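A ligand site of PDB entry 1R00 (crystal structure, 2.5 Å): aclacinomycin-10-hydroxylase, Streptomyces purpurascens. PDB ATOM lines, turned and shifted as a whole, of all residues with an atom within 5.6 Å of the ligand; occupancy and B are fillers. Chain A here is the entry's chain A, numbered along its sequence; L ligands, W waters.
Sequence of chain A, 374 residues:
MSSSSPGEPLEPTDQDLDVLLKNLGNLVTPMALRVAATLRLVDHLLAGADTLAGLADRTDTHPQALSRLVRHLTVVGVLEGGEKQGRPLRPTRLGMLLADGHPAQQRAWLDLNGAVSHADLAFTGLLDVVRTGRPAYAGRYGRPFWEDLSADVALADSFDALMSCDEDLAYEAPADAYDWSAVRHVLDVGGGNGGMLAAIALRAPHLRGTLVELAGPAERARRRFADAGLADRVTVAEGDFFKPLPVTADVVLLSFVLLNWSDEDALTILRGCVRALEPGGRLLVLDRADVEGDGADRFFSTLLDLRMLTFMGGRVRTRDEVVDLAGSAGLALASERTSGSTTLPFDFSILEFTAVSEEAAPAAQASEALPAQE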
ATOM      1  N   TRP A 146      37.854 -18.364  22.580  1.00  0.00           N
ATOM      2  CA  TRP A 146      36.756 -17.459  22.246  1.00  0.00           C
ATOM      3  C   TRP A 146      36.459 -16.445  23.342  1.00  0.00           C
ATOM      4  O   TRP A 146      36.160 -15.288  23.051  1.00  0.00           O
ATOM      5  CB  TRP A 146      35.506 -18.230  21.855  1.00  0.00           C
ATOM      6  CG  TRP A 146      35.693 -18.947  20.609  1.00  0.00           C
ATOM      7  CD1 TRP A 146      35.723 -20.299  20.438  1.00  0.00           C
ATOM      8  CD2 TRP A 146      35.938 -18.379  19.319  1.00  0.00           C
ATOM      9  NE1 TRP A 146      35.943 -20.609  19.123  1.00  0.00           N
ATOM     10  CE2 TRP A 146      36.084 -19.445  18.408  1.00  0.00           C
ATOM     11  CE3 TRP A 146      36.029 -17.063  18.838  1.00  0.00           C
ATOM     12  CZ2 TRP A 146      36.330 -19.245  17.023  1.00  0.00           C
ATOM     13  CZ3 TRP A 146      36.282 -16.855  17.453  1.00  0.00           C
ATOM     14  CH2 TRP A 146      36.415 -17.951  16.568  1.00  0.00           C
ATOM     15  N   CYS A 165      36.003 -15.898   5.597  1.00  0.00           N
ATOM     16  CA  CYS A 165      34.601 -15.650   5.986  1.00  0.00           C
ATOM     17  C   CYS A 165      34.343 -14.184   6.330  1.00  0.00           C
ATOM     18  O   CYS A 165      33.217 -13.707   6.216  1.00  0.00           O
ATOM     19  CB  CYS A 165      34.187 -16.551   7.143  1.00  0.00           C
ATOM     20  SG  CYS A 165      33.960 -18.259   6.609  1.00  0.00           S
ATOM     21  N   TYR A 171      29.237 -14.730   2.424  1.00  0.00           N
ATOM     22  CA  TYR A 171      28.034 -15.487   2.771  1.00  0.00           C
ATOM     23  C   TYR A 171      26.971 -15.479   1.666  1.00  0.00           C
ATOM     24  O   TYR A 171      25.919 -16.059   1.846  1.00  0.00           O
ATOM     25  CB  TYR A 171      27.445 -14.956   4.090  1.00  0.00           C
ATOM     26  CG  TYR A 171      28.341 -15.206   5.266  1.00  0.00           C
ATOM     27  CD1 TYR A 171      29.222 -14.242   5.714  1.00  0.00           C
ATOM     28  CD2 TYR A 171      28.322 -16.427   5.919  1.00  0.00           C
ATOM     29  CE1 TYR A 171      30.074 -14.490   6.797  1.00  0.00           C
ATOM     30  CE2 TYR A 171      29.150 -16.680   6.985  1.00  0.00           C
ATOM     31  CZ  TYR A 171      30.024 -15.710   7.428  1.00  0.00           C
ATOM     32  OH  TYR A 171      30.842 -15.967   8.503  1.00  0.00           O
ATOM     33  N   ASP A 188      20.381 -17.674  15.430  1.00  0.00           N
ATOM     34  CA  ASP A 188      21.708 -17.810  14.870  1.00  0.00           C
ATOM     35  C   ASP A 188      22.639 -18.011  16.065  1.00  0.00           C
ATOM     36  O   ASP A 188      23.047 -17.061  16.740  1.00  0.00           O
ATOM     37  CB  ASP A 188      21.987 -16.527  14.067  1.00  0.00           C
ATOM     38  CG  ASP A 188      23.336 -16.505  13.422  1.00  0.00           C
ATOM     39  OD1 ASP A 188      24.032 -17.549  13.397  1.00  0.00           O
ATOM     40  OD2 ASP A 188      23.784 -15.466  12.895  1.00  0.00           O
ATOM     41  N   VAL A 189      22.923 -19.278  16.385  1.00  0.00           N
ATOM     42  CA  VAL A 189      23.662 -19.600  17.607  1.00  0.00           C
ATOM     43  C   VAL A 189      25.157 -19.473  17.343  1.00  0.00           C
ATOM     44  O   VAL A 189      25.722 -20.234  16.581  1.00  0.00           O
ATOM     45  CB  VAL A 189      23.316 -21.020  18.098  1.00  0.00           C
ATOM     46  CG1 VAL A 189      24.163 -21.417  19.325  1.00  0.00           C
ATOM     47  CG2 VAL A 189      21.846 -21.117  18.416  1.00  0.00           C
ATOM     48  N   GLY A 190      25.795 -18.517  17.996  1.00  0.00           N
ATOM     49  CA  GLY A 190      27.204 -18.228  17.774  1.00  0.00           C
ATOM     50  C   GLY A 190      27.458 -17.530  16.448  1.00  0.00           C
ATOM     51  O   GLY A 190      28.406 -17.844  15.747  1.00  0.00           O
ATOM     52  N   GLY A 191      26.625 -16.545  16.125  1.00  0.00           N
ATOM     53  CA  GLY A 191      26.582 -15.968  14.801  1.00  0.00           C
ATOM     54  C   GLY A 191      27.735 -15.055  14.455  1.00  0.00           C
ATOM     55  O   GLY A 191      27.834 -14.585  13.322  1.00  0.00           O
ATOM     56  N   GLY A 192      28.611 -14.805  15.427  1.00  0.00           N
ATOM     57  CA  GLY A 192      29.769 -13.940  15.241  1.00  0.00           C
ATOM     58  C   GLY A 192      29.295 -12.538  14.991  1.00  0.00           C
ATOM     59  O   GLY A 192      28.397 -12.066  15.683  1.00  0.00           O
ATOM     60  N   ASN A 193      29.841 -11.884  13.976  1.00  0.00           N
ATOM     61  CA  ASN A 193      29.425 -10.522  13.648  1.00  0.00           C
ATOM     62  C   ASN A 193      28.207 -10.454  12.736  1.00  0.00           C
ATOM     63  O   ASN A 193      27.775  -9.363  12.387  1.00  0.00           O
ATOM     64  CB  ASN A 193      30.566  -9.664  13.095  1.00  0.00           C
ATOM     65  CG  ASN A 193      31.435 -10.378  12.114  1.00  0.00           C
ATOM     66  OD1 ASN A 193      32.601 -10.676  12.407  1.00  0.00           O
ATOM     67  ND2 ASN A 193      30.884 -10.695  10.933  1.00  0.00           N
ATOM     68  N   MET A 196      26.322 -14.303   7.852  1.00  0.00           N
ATOM     69  CA  MET A 196      25.278 -15.182   7.334  1.00  0.00           C
ATOM     70  C   MET A 196      23.882 -14.678   7.615  1.00  0.00           C
ATOM     71  O   MET A 196      23.014 -14.800   6.749  1.00  0.00           O
ATOM     72  CB  MET A 196      25.406 -16.594   7.898  1.00  0.00           C
ATOM     73  CG  MET A 196      24.506 -17.605   7.194  1.00  0.00           C
ATOM     74  SD  MET A 196      24.731 -17.625   5.395  1.00  0.00           S
ATOM     75  CE  MET A 196      23.369 -18.728   4.902  1.00  0.00           C
ATOM     76  N   VAL A 212      22.936 -15.074  18.945  1.00  0.00           N
ATOM     77  CA  VAL A 212      23.472 -15.318  20.271  1.00  0.00           C
ATOM     78  C   VAL A 212      24.998 -15.318  20.222  1.00  0.00           C
ATOM     79  O   VAL A 212      25.607 -16.121  19.521  1.00  0.00           O
ATOM     80  CB  VAL A 212      22.979 -16.658  20.875  1.00  0.00           C
ATOM     81  CG1 VAL A 212      23.661 -16.928  22.193  1.00  0.00           C
ATOM     82  CG2 VAL A 212      21.462 -16.654  21.035  1.00  0.00           C
ATOM     83  N   GLU A 213      25.623 -14.407  20.950  1.00  0.00           N
ATOM     84  CA  GLU A 213      27.079 -14.287  20.928  1.00  0.00           C
ATOM     85  C   GLU A 213      27.635 -13.881  22.305  1.00  0.00           C
ATOM     86  O   GLU A 213      26.890 -13.430  23.177  1.00  0.00           O
ATOM     87  CB  GLU A 213      27.488 -13.259  19.874  1.00  0.00           C
ATOM     88  CG  GLU A 213      28.050 -13.833  18.580  1.00  0.00           C
ATOM     89  CD  GLU A 213      29.243 -14.756  18.810  1.00  0.00           C
ATOM     90  OE1 GLU A 213      29.962 -14.538  19.815  1.00  0.00           O
ATOM     91  OE2 GLU A 213      29.462 -15.702  17.985  1.00  0.00           O
ATOM     92  N   LEU A 214      28.932 -14.067  22.487  1.00  0.00           N
ATOM     93  CA  LEU A 214      29.695 -13.384  23.541  1.00  0.00           C
ATOM     94  C   LEU A 214      29.676 -11.887  23.264  1.00  0.00           C
ATOM     95  O   LEU A 214      29.226 -11.466  22.211  1.00  0.00           O
ATOM     96  CB  LEU A 214      31.136 -13.894  23.609  1.00  0.00           C
ATOM     97  CG  LEU A 214      31.253 -15.414  23.816  1.00  0.00           C
ATOM     98  CD1 LEU A 214      32.684 -15.884  23.648  1.00  0.00           C
ATOM     99  CD2 LEU A 214      30.626 -15.833  25.193  1.00  0.00           C
ATOM    100  N   PRO A 217      31.911 -10.188  19.714  1.00  0.00           N
ATOM    101  CA  PRO A 217      31.225 -10.297  18.412  1.00  0.00           C
ATOM    102  C   PRO A 217      29.796  -9.730  18.409  1.00  0.00           C
ATOM    103  O   PRO A 217      29.381  -9.247  17.370  1.00  0.00           O
ATOM    104  CB  PRO A 217      31.247 -11.803  18.120  1.00  0.00           C
ATOM    105  CG  PRO A 217      32.381 -12.325  18.944  1.00  0.00           C
ATOM    106  CD  PRO A 217      32.314 -11.501  20.232  1.00  0.00           C
ATOM    107  N   GLY A 239      24.754 -13.996  25.192  1.00  0.00           N
ATOM    108  CA  GLY A 239      24.359 -15.251  25.815  1.00  0.00           C
ATOM    109  C   GLY A 239      25.454 -16.283  25.725  1.00  0.00           C
ATOM    110  O   GLY A 239      26.464 -16.081  25.096  1.00  0.00           O
ATOM    111  N   ASP A 240      25.220 -17.414  26.375  1.00  0.00           N
ATOM    112  CA  ASP A 240      26.180 -18.500  26.443  1.00  0.00           C
ATOM    113  C   ASP A 240      25.445 -19.708  25.878  1.00  0.00           C
ATOM    114  O   ASP A 240      24.492 -20.182  26.466  1.00  0.00           O
ATOM    115  CB  ASP A 240      26.610 -18.662  27.916  1.00  0.00           C
ATOM    116  CG  ASP A 240      27.568 -19.818  28.169  1.00  0.00           C
ATOM    117  OD1 ASP A 240      28.041 -20.506  27.232  1.00  0.00           O
ATOM    118  OD2 ASP A 240      27.916 -20.104  29.323  1.00  0.00           O
ATOM    119  N   PHE A 241      25.851 -20.180  24.698  1.00  0.00           N
ATOM    120  CA  PHE A 241      25.147 -21.292  24.037  1.00  0.00           C
ATOM    121  C   PHE A 241      25.367 -22.681  24.681  1.00  0.00           C
ATOM    122  O   PHE A 241      24.898 -23.699  24.170  1.00  0.00           O
ATOM    123  CB  PHE A 241      25.363 -21.307  22.498  1.00  0.00           C
ATOM    124  CG  PHE A 241      26.789 -21.454  22.030  1.00  0.00           C
ATOM    125  CD1 PHE A 241      27.704 -22.275  22.683  1.00  0.00           C
ATOM    126  CD2 PHE A 241      27.208 -20.790  20.870  1.00  0.00           C
ATOM    127  CE1 PHE A 241      29.003 -22.399  22.187  1.00  0.00           C
ATOM    128  CE2 PHE A 241      28.497 -20.918  20.383  1.00  0.00           C
ATOM    129  CZ  PHE A 241      29.397 -21.711  21.033  1.00  0.00           C
ATOM    130  N   PHE A 242      26.071 -22.697  25.818  1.00  0.00           N
ATOM    131  CA  PHE A 242      26.016 -23.807  26.766  1.00  0.00           C
ATOM    132  C   PHE A 242      24.849 -23.676  27.756  1.00  0.00           C
ATOM    133  O   PHE A 242      24.365 -24.695  28.298  1.00  0.00           O
ATOM    134  CB  PHE A 242      27.363 -23.951  27.503  1.00  0.00           C
ATOM    135  CG  PHE A 242      28.473 -24.317  26.587  1.00  0.00           C
ATOM    136  CD1 PHE A 242      29.473 -23.413  26.279  1.00  0.00           C
ATOM    137  CD2 PHE A 242      28.491 -25.542  25.977  1.00  0.00           C
ATOM    138  CE1 PHE A 242      30.491 -23.762  25.414  1.00  0.00           C
ATOM    139  CE2 PHE A 242      29.502 -25.885  25.108  1.00  0.00           C
ATOM    140  CZ  PHE A 242      30.503 -24.981  24.823  1.00  0.00           C
ATOM    141  N   SER A 255      26.443 -21.664  12.060  1.00  0.00           N
ATOM    142  CA  SER A 255      27.319 -21.344  10.931  1.00  0.00           C
ATOM    143  C   SER A 255      28.799 -21.280  11.364  1.00  0.00           C
ATOM    144  O   SER A 255      29.214 -20.337  12.065  1.00  0.00           O
ATOM    145  CB  SER A 255      26.890 -20.019  10.258  1.00  0.00           C
ATOM    146  OG  SER A 255      27.929 -19.500   9.410  1.00  0.00           O
ATOM    147  N   PHE A 256      29.571 -22.281  10.923  1.00  0.00           N
ATOM    148  CA  PHE A 256      30.981 -22.465  11.286  1.00  0.00           C
ATOM    149  C   PHE A 256      31.176 -22.366  12.754  1.00  0.00           C
ATOM    150  O   PHE A 256      32.052 -21.645  13.208  1.00  0.00           O
ATOM    151  CB  PHE A 256      31.902 -21.467  10.549  1.00  0.00           C
ATOM    152  CG  PHE A 256      31.757 -21.545   9.081  1.00  0.00           C
ATOM    153  CD1 PHE A 256      31.063 -20.588   8.374  1.00  0.00           C
ATOM    154  CD2 PHE A 256      32.280 -22.638   8.395  1.00  0.00           C
ATOM    155  CE1 PHE A 256      30.904 -20.680   7.005  1.00  0.00           C
ATOM    156  CE2 PHE A 256      32.133 -22.742   7.034  1.00  0.00           C
ATOM    157  CZ  PHE A 256      31.437 -21.755   6.328  1.00  0.00           C
ATOM    158  N   VAL A 257      30.364 -23.110  13.506  1.00  0.00           N
ATOM    159  CA  VAL A 257      30.486 -23.175  14.965  1.00  0.00           C
ATOM    160  C   VAL A 257      30.948 -24.543  15.498  1.00  0.00           C
ATOM    161  O   VAL A 257      31.816 -24.613  16.390  1.00  0.00           O
ATOM    162  CB  VAL A 257      29.155 -22.805  15.639  1.00  0.00           C
ATOM    163  CG1 VAL A 257      29.246 -22.952  17.168  1.00  0.00           C
ATOM    164  CG2 VAL A 257      28.753 -21.386  15.232  1.00  0.00           C
ATOM    165  N   ASN A 260      34.683 -25.884  15.913  1.00  0.00           N
ATOM    166  CA  ASN A 260      35.461 -25.379  17.038  1.00  0.00           C
ATOM    167  C   ASN A 260      35.335 -26.169  18.359  1.00  0.00           C
ATOM    168  O   ASN A 260      35.914 -25.766  19.359  1.00  0.00           O
ATOM    169  CB  ASN A 260      35.073 -23.930  17.419  1.00  0.00           C
ATOM    170  CG  ASN A 260      35.078 -22.948  16.240  1.00  0.00           C
ATOM    171  OD1 ASN A 260      34.256 -22.031  16.228  1.00  0.00           O
ATOM    172  ND2 ASN A 260      35.999 -23.096  15.302  1.00  0.00           N
ATOM    173  N   TRP A 261      34.551 -27.230  18.403  1.00  0.00           N
ATOM    174  CA  TRP A 261      34.238 -27.845  19.706  1.00  0.00           C
ATOM    175  C   TRP A 261      34.429 -29.335  19.698  1.00  0.00           C
ATOM    176  O   TRP A 261      34.331 -29.954  18.666  1.00  0.00           O
ATOM    177  CB  TRP A 261      32.813 -27.480  20.162  1.00  0.00           C
ATOM    178  CG  TRP A 261      32.676 -26.043  20.391  1.00  0.00           C
ATOM    179  CD1 TRP A 261      32.149 -25.130  19.546  1.00  0.00           C
ATOM    180  CD2 TRP A 261      33.128 -25.318  21.546  1.00  0.00           C
ATOM    181  NE1 TRP A 261      32.214 -23.873  20.097  1.00  0.00           N
ATOM    182  CE2 TRP A 261      32.805 -23.948  21.324  1.00  0.00           C
ATOM    183  CE3 TRP A 261      33.759 -25.677  22.741  1.00  0.00           C
ATOM    184  CZ2 TRP A 261      33.112 -22.948  22.257  1.00  0.00           C
ATOM    185  CZ3 TRP A 261      34.046 -24.672  23.666  1.00  0.00           C
ATOM    186  CH2 TRP A 261      33.728 -23.333  23.411  1.00  0.00           C
HETATM  187  N1  LIG L   1      28.545 -17.894  12.960  1.00  0.00           N
HETATM  188  C1  LIG L   1      29.848 -17.274  12.777  1.00  0.00           C
HETATM  189  C2  LIG L   1      30.864 -18.068  13.599  1.00  0.00           C
HETATM  190  C3  LIG L   1      31.972 -17.236  14.209  1.00  0.00           C
HETATM  191  S1  LIG L   1      33.238 -18.344  14.861  1.00  0.00           S
HETATM  192  C4  LIG L   1      30.295 -17.315  11.314  1.00  0.00           C
HETATM  193  O1  LIG L   1      29.478 -17.484  10.392  1.00  0.00           O
HETATM  194  O2  LIG L   1      31.489 -17.221  11.045  1.00  0.00           O
HETATM  195  C5  LIG L   1      32.441 -19.015  16.345  1.00  0.00           C
HETATM  196  C6  LIG L   1      31.744 -18.024  17.299  1.00  0.00           C
HETATM  197  O3  LIG L   1      31.320 -18.752  18.444  1.00  0.00           O
HETATM  198  C7  LIG L   1      32.600 -16.888  17.829  1.00  0.00           C
HETATM  199  O4  LIG L   1      32.101 -15.638  17.418  1.00  0.00           O
HETATM  200  C8  LIG L   1      32.505 -16.998  19.348  1.00  0.00           C
HETATM  201  O5  LIG L   1      32.371 -15.760  19.969  1.00  0.00           O
HETATM  202  C9  LIG L   1      31.284 -17.886  19.553  1.00  0.00           C
HETATM  203  N2  LIG L   1      31.234 -18.568  20.867  1.00  0.00           N
HETATM  204  C10 LIG L   1      32.183 -19.338  21.472  1.00  0.00           C
HETATM  205  N3  LIG L   1      31.689 -19.755  22.663  1.00  0.00           N
HETATM  206  C11 LIG L   1      30.445 -19.254  22.843  1.00  0.00           C
HETATM  207  C12 LIG L   1      29.474 -19.362  23.863  1.00  0.00           C
HETATM  208  N4  LIG L   1      29.671 -20.039  25.007  1.00  0.00           N
HETATM  209  N5  LIG L   1      28.281 -18.712  23.706  1.00  0.00           N
HETATM  210  C13 LIG L   1      28.008 -17.964  22.570  1.00  0.00           C
HETATM  211  N6  LIG L   1      28.959 -17.880  21.571  1.00  0.00           N
HETATM  212  C14 LIG L   1      30.156 -18.505  21.711  1.00  0.00           C
HETATM  213  O   HOH W   1      33.508 -18.178   9.411  1.00  0.00           O
HETATM  214  O   HOH W   2      34.827 -14.244  20.612  1.00  0.00           O
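The backbone NH of Gly 190 lies within hydrogen-bond range of the backbone carbonyl oxygen of Val 212 (2.8 Å).
The backbone NH (N) of Gly 192 lies within hydrogen-bond range of the side-chain carboxylate (OE2) of Glu 213 (2.8 Å).
The backbone carbonyl oxygen (O) of Glu 213 is in hydrogen-bond range of the backbone NH (N) of Gly 239, 3.0 Å away.
OE2 of Glu 213 is in hydrogen-bond range of N of Gly 191 (3.5 Å).
The backbone NH (N) of Phe 242 lies close to the side-chain carboxylate (OD1) of Asp 240, at 3.3 Å.
The backbone carbonyl oxygen (O) of Gly 191 sits close to a nitrogen (N1) of the ligand (3.4 Å).
N5 of the ligand lies within hydrogen-bond range of N of Phe 241.
The side-chain carboxylate of Glu 213 is in hydrogen-bond range of an oxygen (O4) of the ligand (2.7 Å).
O of Ser 255 lies within hydrogen-bond range of N1 of the ligand.
The side-chain carboxylate (OD1) of Asp 240 lies within hydrogen-bond range of a nitrogen (N4) of the ligand, 2.8 Å away.
An oxygen (O1) of the ligand lies within hydrogen-bond range of the side-chain hydroxyl (OH) of Tyr 171.
A nitrogen (N1) of the ligand lies within hydrogen-bond range of the backbone carbonyl oxygen (O) of Gly 190.
The side-chain hydroxyl of Ser 255 lies within hydrogen-bond range of an oxygen (O1) of the ligand (2.7 Å).
O of Gly 239 sits close to N5 of the ligand (3.5 Å).
Trp 146 touches the ligand.
Gly 192 touches the ligand.
Leu 214 touches the ligand (CD1 to O5, 3.7 Å).
Pro 217 touches the ligand.
Phe 242 touches the ligand (CD1 to N4, 3.6 Å).
O of Phe 256 touches C2 of the ligand, at 3.8 Å.
OD1 of Asn 260 touches C5 of the ligand, at 3.5 Å.
CZ2 of Trp 261 touches N3 of the ligand, at 3.5 Å.
Hydrophobic or aromatic side chains that line the ligand: Trp 146, Tyr 171, Leu 214, Pro 217, Phe 241, Phe 242 and Trp 261.
16 residues have an atom within 4 Å of the ligand: Trp 146, Tyr 171, Gly 190, Gly 191, Gly 192, Glu 213, Leu 214, Pro 217, Gly 239, Asp 240, Phe 241, Phe 242, Ser 255, Phe 256, Asn 260 and Trp 261.
Water W1 lies within hydrogen-bond range of an oxygen (O2) of the ligand (2.8 Å) and the side-chain sulfur (SG) of Cys 165 (2.8 Å).
Water W2 lies within hydrogen-bond range of an oxygen (O5) of the ligand (3.0 Å) and the backbone carbonyl oxygen of Trp 146 (3.0 Å).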
